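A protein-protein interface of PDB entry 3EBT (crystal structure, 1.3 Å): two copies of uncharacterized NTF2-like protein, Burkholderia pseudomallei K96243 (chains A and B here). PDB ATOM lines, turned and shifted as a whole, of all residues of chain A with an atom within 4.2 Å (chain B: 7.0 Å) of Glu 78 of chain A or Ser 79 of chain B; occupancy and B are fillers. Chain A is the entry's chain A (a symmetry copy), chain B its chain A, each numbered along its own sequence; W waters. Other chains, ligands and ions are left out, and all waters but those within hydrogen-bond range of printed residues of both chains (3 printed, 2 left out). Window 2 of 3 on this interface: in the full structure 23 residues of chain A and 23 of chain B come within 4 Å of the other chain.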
ATOM      1  N   SER A   3     -19.829  13.432  -8.587  1.00  0.00           N
ATOM      2  CA  SER A   3     -19.213  13.379  -9.903  1.00  0.00           C
ATOM      3  C   SER A   3     -17.737  13.761  -9.804  1.00  0.00           C
ATOM      4  O   SER A   3     -17.306  14.432  -8.856  1.00  0.00           O
ATOM      5  CB  SER A   3     -19.900  14.333 -10.873  1.00  0.00           C
ATOM      6  OG  SER A   3     -19.516  15.675 -10.577  1.00  0.00           O
ATOM      7  N   MET A   6     -17.400  17.536  -9.730  1.00  0.00           N
ATOM      8  CA  MET A   6     -17.691  18.079  -8.415  1.00  0.00           C
ATOM      9  C   MET A   6     -16.472  17.900  -7.504  1.00  0.00           C
ATOM     10  O   MET A   6     -16.097  18.798  -6.780  1.00  0.00           O
ATOM     11  CB  MET A   6     -18.963  17.450  -7.838  1.00  0.00           C
ATOM     12  CG  MET A   6     -19.368  17.967  -6.513  1.00  0.00           C
ATOM     13  SD  MET A   6     -19.869  19.847  -6.601  1.00  0.00           S
ATOM     14  CE  MET A   6     -21.744  19.615  -7.221  1.00  0.00           C
ATOM     15  N   PHE A  76     -23.244  24.304  -3.964  1.00  0.00           N
ATOM     16  CA  PHE A  76     -22.652  23.770  -5.198  1.00  0.00           C
ATOM     17  C   PHE A  76     -23.831  23.255  -6.032  1.00  0.00           C
ATOM     18  O   PHE A  76     -24.546  22.355  -5.584  1.00  0.00           O
ATOM     19  CB  PHE A  76     -21.676  22.633  -4.889  1.00  0.00           C
ATOM     20  CG  PHE A  76     -20.449  23.056  -4.121  1.00  0.00           C
ATOM     21  CD1 PHE A  76     -20.492  23.242  -2.746  1.00  0.00           C
ATOM     22  CD2 PHE A  76     -19.228  23.217  -4.769  1.00  0.00           C
ATOM     23  CE1 PHE A  76     -19.349  23.610  -2.037  1.00  0.00           C
ATOM     24  CE2 PHE A  76     -18.082  23.557  -4.066  1.00  0.00           C
ATOM     25  CZ  PHE A  76     -18.149  23.762  -2.694  1.00  0.00           C
ATOM     26  N   ILE A  77     -24.029  23.835  -7.207  1.00  0.00           N
ATOM     27  CA  ILE A  77     -25.170  23.581  -8.068  1.00  0.00           C
ATOM     28  C   ILE A  77     -24.658  23.070  -9.407  1.00  0.00           C
ATOM     29  O   ILE A  77     -24.111  23.831 -10.202  1.00  0.00           O
ATOM     30  CB  ILE A  77     -25.975  24.879  -8.229  1.00  0.00           C
ATOM     31  CG1 ILE A  77     -26.467  25.382  -6.852  1.00  0.00           C
ATOM     32  CG2 ILE A  77     -27.133  24.707  -9.216  1.00  0.00           C
ATOM     33  CD1 ILE A  77     -27.065  26.801  -6.890  1.00  0.00           C
ATOM     34  N   GLU A  78     -24.837  21.771  -9.631  1.00  0.00           N
ATOM     35  CA  GLU A  78     -24.300  21.097 -10.830  1.00  0.00           C
ATOM     36  C   GLU A  78     -25.405  20.653 -11.753  1.00  0.00           C
ATOM     37  O   GLU A  78     -26.406  20.066 -11.307  1.00  0.00           O
ATOM     38  CB  GLU A  78     -23.534  19.869 -10.381  1.00  0.00           C
ATOM     39  CG  GLU A  78     -22.914  19.006 -11.479  1.00  0.00           C
ATOM     40  CD  GLU A  78     -22.120  17.860 -10.920  1.00  0.00           C
ATOM     41  OE1 GLU A  78     -22.473  17.291  -9.870  1.00  0.00           O
ATOM     42  OE2 GLU A  78     -21.087  17.511 -11.536  1.00  0.00           O
ATOM     43  N   SER A  79     -25.217  20.922 -13.037  1.00  0.00           N
ATOM     44  CA  SER A  79     -26.068  20.401 -14.086  1.00  0.00           C
ATOM     45  C   SER A  79     -25.215  20.127 -15.302  1.00  0.00           C
ATOM     46  O   SER A  79     -24.614  21.050 -15.845  1.00  0.00           O
ATOM     47  CB  SER A  79     -27.173  21.371 -14.442  1.00  0.00           C
ATOM     48  OG  SER A  79     -27.991  20.852 -15.465  1.00  0.00           O
ATOM     49  N   GLY A  80     -25.169  18.871 -15.737  1.00  0.00           N
ATOM     50  CA  GLY A  80     -24.322  18.511 -16.862  1.00  0.00           C
ATOM     51  C   GLY A  80     -22.875  18.811 -16.469  1.00  0.00           C
ATOM     52  O   GLY A  80     -22.418  18.448 -15.374  1.00  0.00           O
ATOM     53  N   ARG A  82     -21.680  21.890 -16.059  1.00  0.00           N
ATOM     54  CA  ARG A  82     -21.619  23.183 -15.403  1.00  0.00           C
ATOM     55  C   ARG A  82     -21.769  23.038 -13.904  1.00  0.00           C
ATOM     56  O   ARG A  82     -22.632  22.288 -13.457  1.00  0.00           O
ATOM     57  CB  ARG A  82     -22.751  24.086 -15.870  1.00  0.00           C
ATOM     58  CG  ARG A  82     -22.846  24.333 -17.369  1.00  0.00           C
ATOM     59  CD  ARG A  82     -23.588  23.268 -18.145  1.00  0.00           C
ATOM     60  NE  ARG A  82     -24.968  23.018 -17.688  1.00  0.00           N
ATOM     61  CZ  ARG A  82     -26.030  23.731 -18.006  1.00  0.00           C
ATOM     62  NH1 ARG A  82     -25.951  24.817 -18.770  1.00  0.00           N
ATOM     63  NH2 ARG A  82     -27.224  23.341 -17.533  1.00  0.00           N
ATOM     64  N   ILE A  83     -20.962  23.774 -13.130  1.00  0.00           N
ATOM     65  CA  ILE A  83     -21.082  23.835 -11.681  1.00  0.00           C
ATOM     66  C   ILE A  83     -21.024  25.307 -11.265  1.00  0.00           C
ATOM     67  O   ILE A  83     -20.080  26.004 -11.608  1.00  0.00           O
ATOM     68  CB  ILE A  83     -20.031  23.016 -10.951  1.00  0.00           C
ATOM     69  CG1 ILE A  83     -20.147  21.516 -11.332  1.00  0.00           C
ATOM     70  CG2 ILE A  83     -20.220  23.178  -9.434  1.00  0.00           C
ATOM     71  CD1 ILE A  83     -19.088  20.600 -10.762  1.00  0.00           C
ATOM     72  N   MET B   6     -38.422  24.938 -13.543  1.00  0.00           N
ATOM     73  CA  MET B   6     -37.775  25.474 -14.727  1.00  0.00           C
ATOM     74  C   MET B   6     -38.797  26.247 -15.566  1.00  0.00           C
ATOM     75  O   MET B   6     -38.521  27.323 -16.051  1.00  0.00           O
ATOM     76  CB  MET B   6     -37.078  24.360 -15.515  1.00  0.00           C
ATOM     77  CG  MET B   6     -36.353  24.811 -16.723  1.00  0.00           C
ATOM     78  SD  MET B   6     -34.852  25.963 -16.268  1.00  0.00           S
ATOM     79  CE  MET B   6     -33.520  24.547 -15.848  1.00  0.00           C
ATOM     80  N   ILE B  77     -29.198  26.498 -15.116  1.00  0.00           N
ATOM     81  CA  ILE B  77     -28.490  25.444 -14.412  1.00  0.00           C
ATOM     82  C   ILE B  77     -29.297  25.059 -13.182  1.00  0.00           C
ATOM     83  O   ILE B  77     -29.347  25.802 -12.205  1.00  0.00           O
ATOM     84  CB  ILE B  77     -27.089  25.949 -14.033  1.00  0.00           C
ATOM     85  CG1 ILE B  77     -26.299  26.348 -15.301  1.00  0.00           C
ATOM     86  CG2 ILE B  77     -26.327  24.922 -13.191  1.00  0.00           C
ATOM     87  CD1 ILE B  77     -24.986  27.096 -15.001  1.00  0.00           C
ATOM     88  N   GLU B  78     -29.932  23.892 -13.256  1.00  0.00           N
ATOM     89  CA  GLU B  78     -30.846  23.424 -12.196  1.00  0.00           C
ATOM     90  C   GLU B  78     -30.283  22.229 -11.470  1.00  0.00           C
ATOM     91  O   GLU B  78     -29.788  21.279 -12.102  1.00  0.00           O
ATOM     92  CB  GLU B  78     -32.154  23.013 -12.843  1.00  0.00           C
ATOM     93  CG  GLU B  78     -33.238  22.468 -11.915  1.00  0.00           C
ATOM     94  CD  GLU B  78     -34.512  22.161 -12.650  1.00  0.00           C
ATOM     95  OE1 GLU B  78     -34.487  21.736 -13.820  1.00  0.00           O
ATOM     96  OE2 GLU B  78     -35.594  22.364 -12.052  1.00  0.00           O
ATOM     97  N   SER B  79     -30.367  22.273 -10.149  1.00  0.00           N
ATOM     98  CA  SER B  79     -30.062  21.141  -9.300  1.00  0.00           C
ATOM     99  C   SER B  79     -30.997  21.166  -8.114  1.00  0.00           C
ATOM    100  O   SER B  79     -30.978  22.122  -7.343  1.00  0.00           O
ATOM    101  CB  SER B  79     -28.626  21.171  -8.823  1.00  0.00           C
ATOM    102  OG  SER B  79     -28.345  20.065  -7.996  1.00  0.00           O
ATOM    103  N   GLY B  80     -31.804  20.120  -7.957  1.00  0.00           N
ATOM    104  CA  GLY B  80     -32.777  20.095  -6.879  1.00  0.00           C
ATOM    105  C   GLY B  80     -33.739  21.265  -7.094  1.00  0.00           C
ATOM    106  O   GLY B  80     -34.243  21.485  -8.206  1.00  0.00           O
ATOM    107  N   GLU B  81     -33.944  22.017  -6.034  1.00  0.00           N
ATOM    108  CA  GLU B  81     -34.839  23.180  -6.027  1.00  0.00           C
ATOM    109  C   GLU B  81     -34.124  24.508  -6.278  1.00  0.00           C
ATOM    110  O   GLU B  81     -34.726  25.561  -6.081  1.00  0.00           O
ATOM    111  CB  GLU B  81     -35.654  23.179  -4.742  1.00  0.00           C
ATOM    112  CG  GLU B  81     -36.772  22.154  -4.768  1.00  0.00           C
ATOM    113  CD  GLU B  81     -37.501  22.043  -3.449  1.00  0.00           C
ATOM    114  OE1 GLU B  81     -36.941  21.482  -2.498  1.00  0.00           O
ATOM    115  OE2 GLU B  81     -38.667  22.492  -3.371  1.00  0.00           O
ATOM    116  N   ARG B  82     -32.863  24.456  -6.745  1.00  0.00           N
ATOM    117  CA  ARG B  82     -32.106  25.642  -7.101  1.00  0.00           C
ATOM    118  C   ARG B  82     -31.964  25.763  -8.603  1.00  0.00           C
ATOM    119  O   ARG B  82     -31.678  24.767  -9.262  1.00  0.00           O
ATOM    120  CB  ARG B  82     -30.697  25.580  -6.532  1.00  0.00           C
ATOM    121  CG  ARG B  82     -30.581  25.394  -5.026  1.00  0.00           C
ATOM    122  CD  ARG B  82     -30.664  23.960  -4.553  1.00  0.00           C
ATOM    123  NE  ARG B  82     -29.666  23.052  -5.150  1.00  0.00           N
ATOM    124  CZ  ARG B  82     -28.414  22.916  -4.762  1.00  0.00           C
ATOM    125  NH1 ARG B  82     -27.894  23.645  -3.778  1.00  0.00           N
ATOM    126  NH2 ARG B  82     -27.648  22.012  -5.392  1.00  0.00           N
ATOM    127  N   ILE B  83     -32.127  26.978  -9.141  1.00  0.00           N
ATOM    128  CA  ILE B  83     -31.891  27.267 -10.548  1.00  0.00           C
ATOM    129  C   ILE B  83     -31.043  28.539 -10.633  1.00  0.00           C
ATOM    130  O   ILE B  83     -31.419  29.563 -10.081  1.00  0.00           O
ATOM    131  CB  ILE B  83     -33.167  27.403 -11.361  1.00  0.00           C
ATOM    132  CG1 ILE B  83     -33.983  26.083 -11.321  1.00  0.00           C
ATOM    133  CG2 ILE B  83     -32.812  27.745 -12.816  1.00  0.00           C
ATOM    134  CD1 ILE B  83     -35.334  26.114 -11.998  1.00  0.00           C
ATOM    135  N   VAL B  84     -29.936  28.453 -11.362  1.00  0.00           N
ATOM    136  CA  VAL B  84     -29.070  29.603 -11.638  1.00  0.00           C
ATOM    137  C   VAL B  84     -29.225  29.924 -13.108  1.00  0.00           C
ATOM    138  O   VAL B  84     -29.152  29.036 -13.973  1.00  0.00           O
ATOM    139  CB  VAL B  84     -27.615  29.335 -11.300  1.00  0.00           C
ATOM    140  CG1 VAL B  84     -26.745  30.564 -11.621  1.00  0.00           C
ATOM    141  CG2 VAL B  84     -27.458  28.959  -9.837  1.00  0.00           C
HETATM  142  O   HOH W   1     -25.243  22.784  -2.362  1.00  0.00           O
HETATM  143  O   HOH W   2     -30.135  22.447 -15.785  1.00  0.00           O
HETATM  144  O   HOH W   3     -25.703  19.980  -7.494  1.00  0.00           O
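Among the printed residues, merely in contact across the chains: Ile 77 of chain A with Ile 77 of chain B, Ile 77 of chain A with Ser 79 of chain B, Ile 77 of chain A with Arg 82 of chain B, Ile 77 of chain A with Val 84 of chain B, Glu 78 of chain A with Glu 78 of chain B, Glu 78 of chain A with Ser 79 of chain B, Ser 79 of chain A with Ile 77 of chain B, Ser 79 of chain A with Glu 78 of chain B and Arg 82 of chain A with Ile 77 of chain B.
Printed residues of chain A that touch a printed residue of chain B: Phe 76, Ile 77, Glu 78, Ser 79 and Arg 82. Printed residues of chain B that touch a printed residue of chain A: Ile 77, Glu 78, Ser 79, Arg 82 and Val 84. Hydrophobic or aromatic side chains of chain B within 4 Å of the printed part of chain A: Ile 77 and Val 84. Among the printed residues, 10 pairs touch across the chains. Among the printed residues, no Asp or Glu carboxylate lies within 4 Å of a Lys or Arg side-chain nitrogen of the other chain.
NH2 of Arg 82 of chain B sits at hydrogen-bond distance from O of Phe 76 of chain A, 3.1 Å away.
Glu 78 of chain A touches just these residues of chain B: Glu 78 and Ser 79. Of chain A, only Ile 77 (3.9 Å) and Glu 78 (3.5 Å) come within 4 Å of Ser 79 of chain B. Of the printed residues of chain B, Ser 79 of chain A touches Ile 77 (3.9 Å) and Glu 78 (3.5 Å). Of the printed residues of chain A, Val 84 of chain B touches Ile 77 (3.7 Å). Of the printed residues of chain A, Ile 77 of chain B touches Ile 77 (3.9 Å), Ser 79 (3.9 Å) and Arg 82 (3.8 Å). Printed residues of chain B within 4 Å of Arg 82 of chain A: Ile 77 (3.8 Å). The nearest printed residue of chain A that does not touch Ser 79 of chain B is Phe 76 of chain A (5.0 Å). The nearest printed residue of chain A that does not touch Arg 82 of chain B is Glu 78 of chain A (5.1 Å).
Ile 77 of chain B touches its own counterpart, Ile 77 of chain A. Ile 77 of chain A touches Ser 79 of chain B, and with the chains exchanged Ser 79 of chain A touches Ile 77 of chain B. Ile 77 of chain A touches Arg 82 of chain B, and with the chains exchanged Arg 82 of chain A touches Ile 77 of chain B. Glu 78 of chain A touches Ser 79 of chain B, and with the chains exchanged Ser 79 of chain A touches Glu 78 of chain B. Positions printed for both chains: 6, 77, 78, 79, 80, 82 and 83. Of the 10 pairs that touch across the chains among the printed residues, 8 have their exchanged pair printed and touching as well.
The side-chain hydroxyl (OG) of Ser 3 of chain A lies within hydrogen-bond range of the side-chain carboxylate (OE2) of Glu 78 of chain A, at 2.6 Å. NE of Arg 82 of chain A sits at hydrogen-bond distance from O of Ser 79 of chain A, at 2.7 Å. N of Ile 77 of chain B sits at hydrogen-bond distance from O of Val 84 of chain B, at 2.8 Å. NE of Arg 82 of chain B sits at hydrogen-bond distance from O of Ser 79 of chain B (2.7 Å).
Water W2 bridges the side-chain hydroxyl (OG) of Ser 79 of chain A (2.7 Å) and the backbone NH (N) of Glu 78 of chain B (2.9 Å). Water W3 lies within hydrogen-bond range of the side-chain hydroxyl of Ser 79 of chain B (2.7 Å), the backbone NH of Glu 78 of chain A (2.9 Å) and the backbone carbonyl oxygen of Phe 76 of chain A (3.3 Å). Water W1 bridges N of Phe 76 of chain A (3.0 Å) and NH1 of Arg 82 of chain B (3.1 Å).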
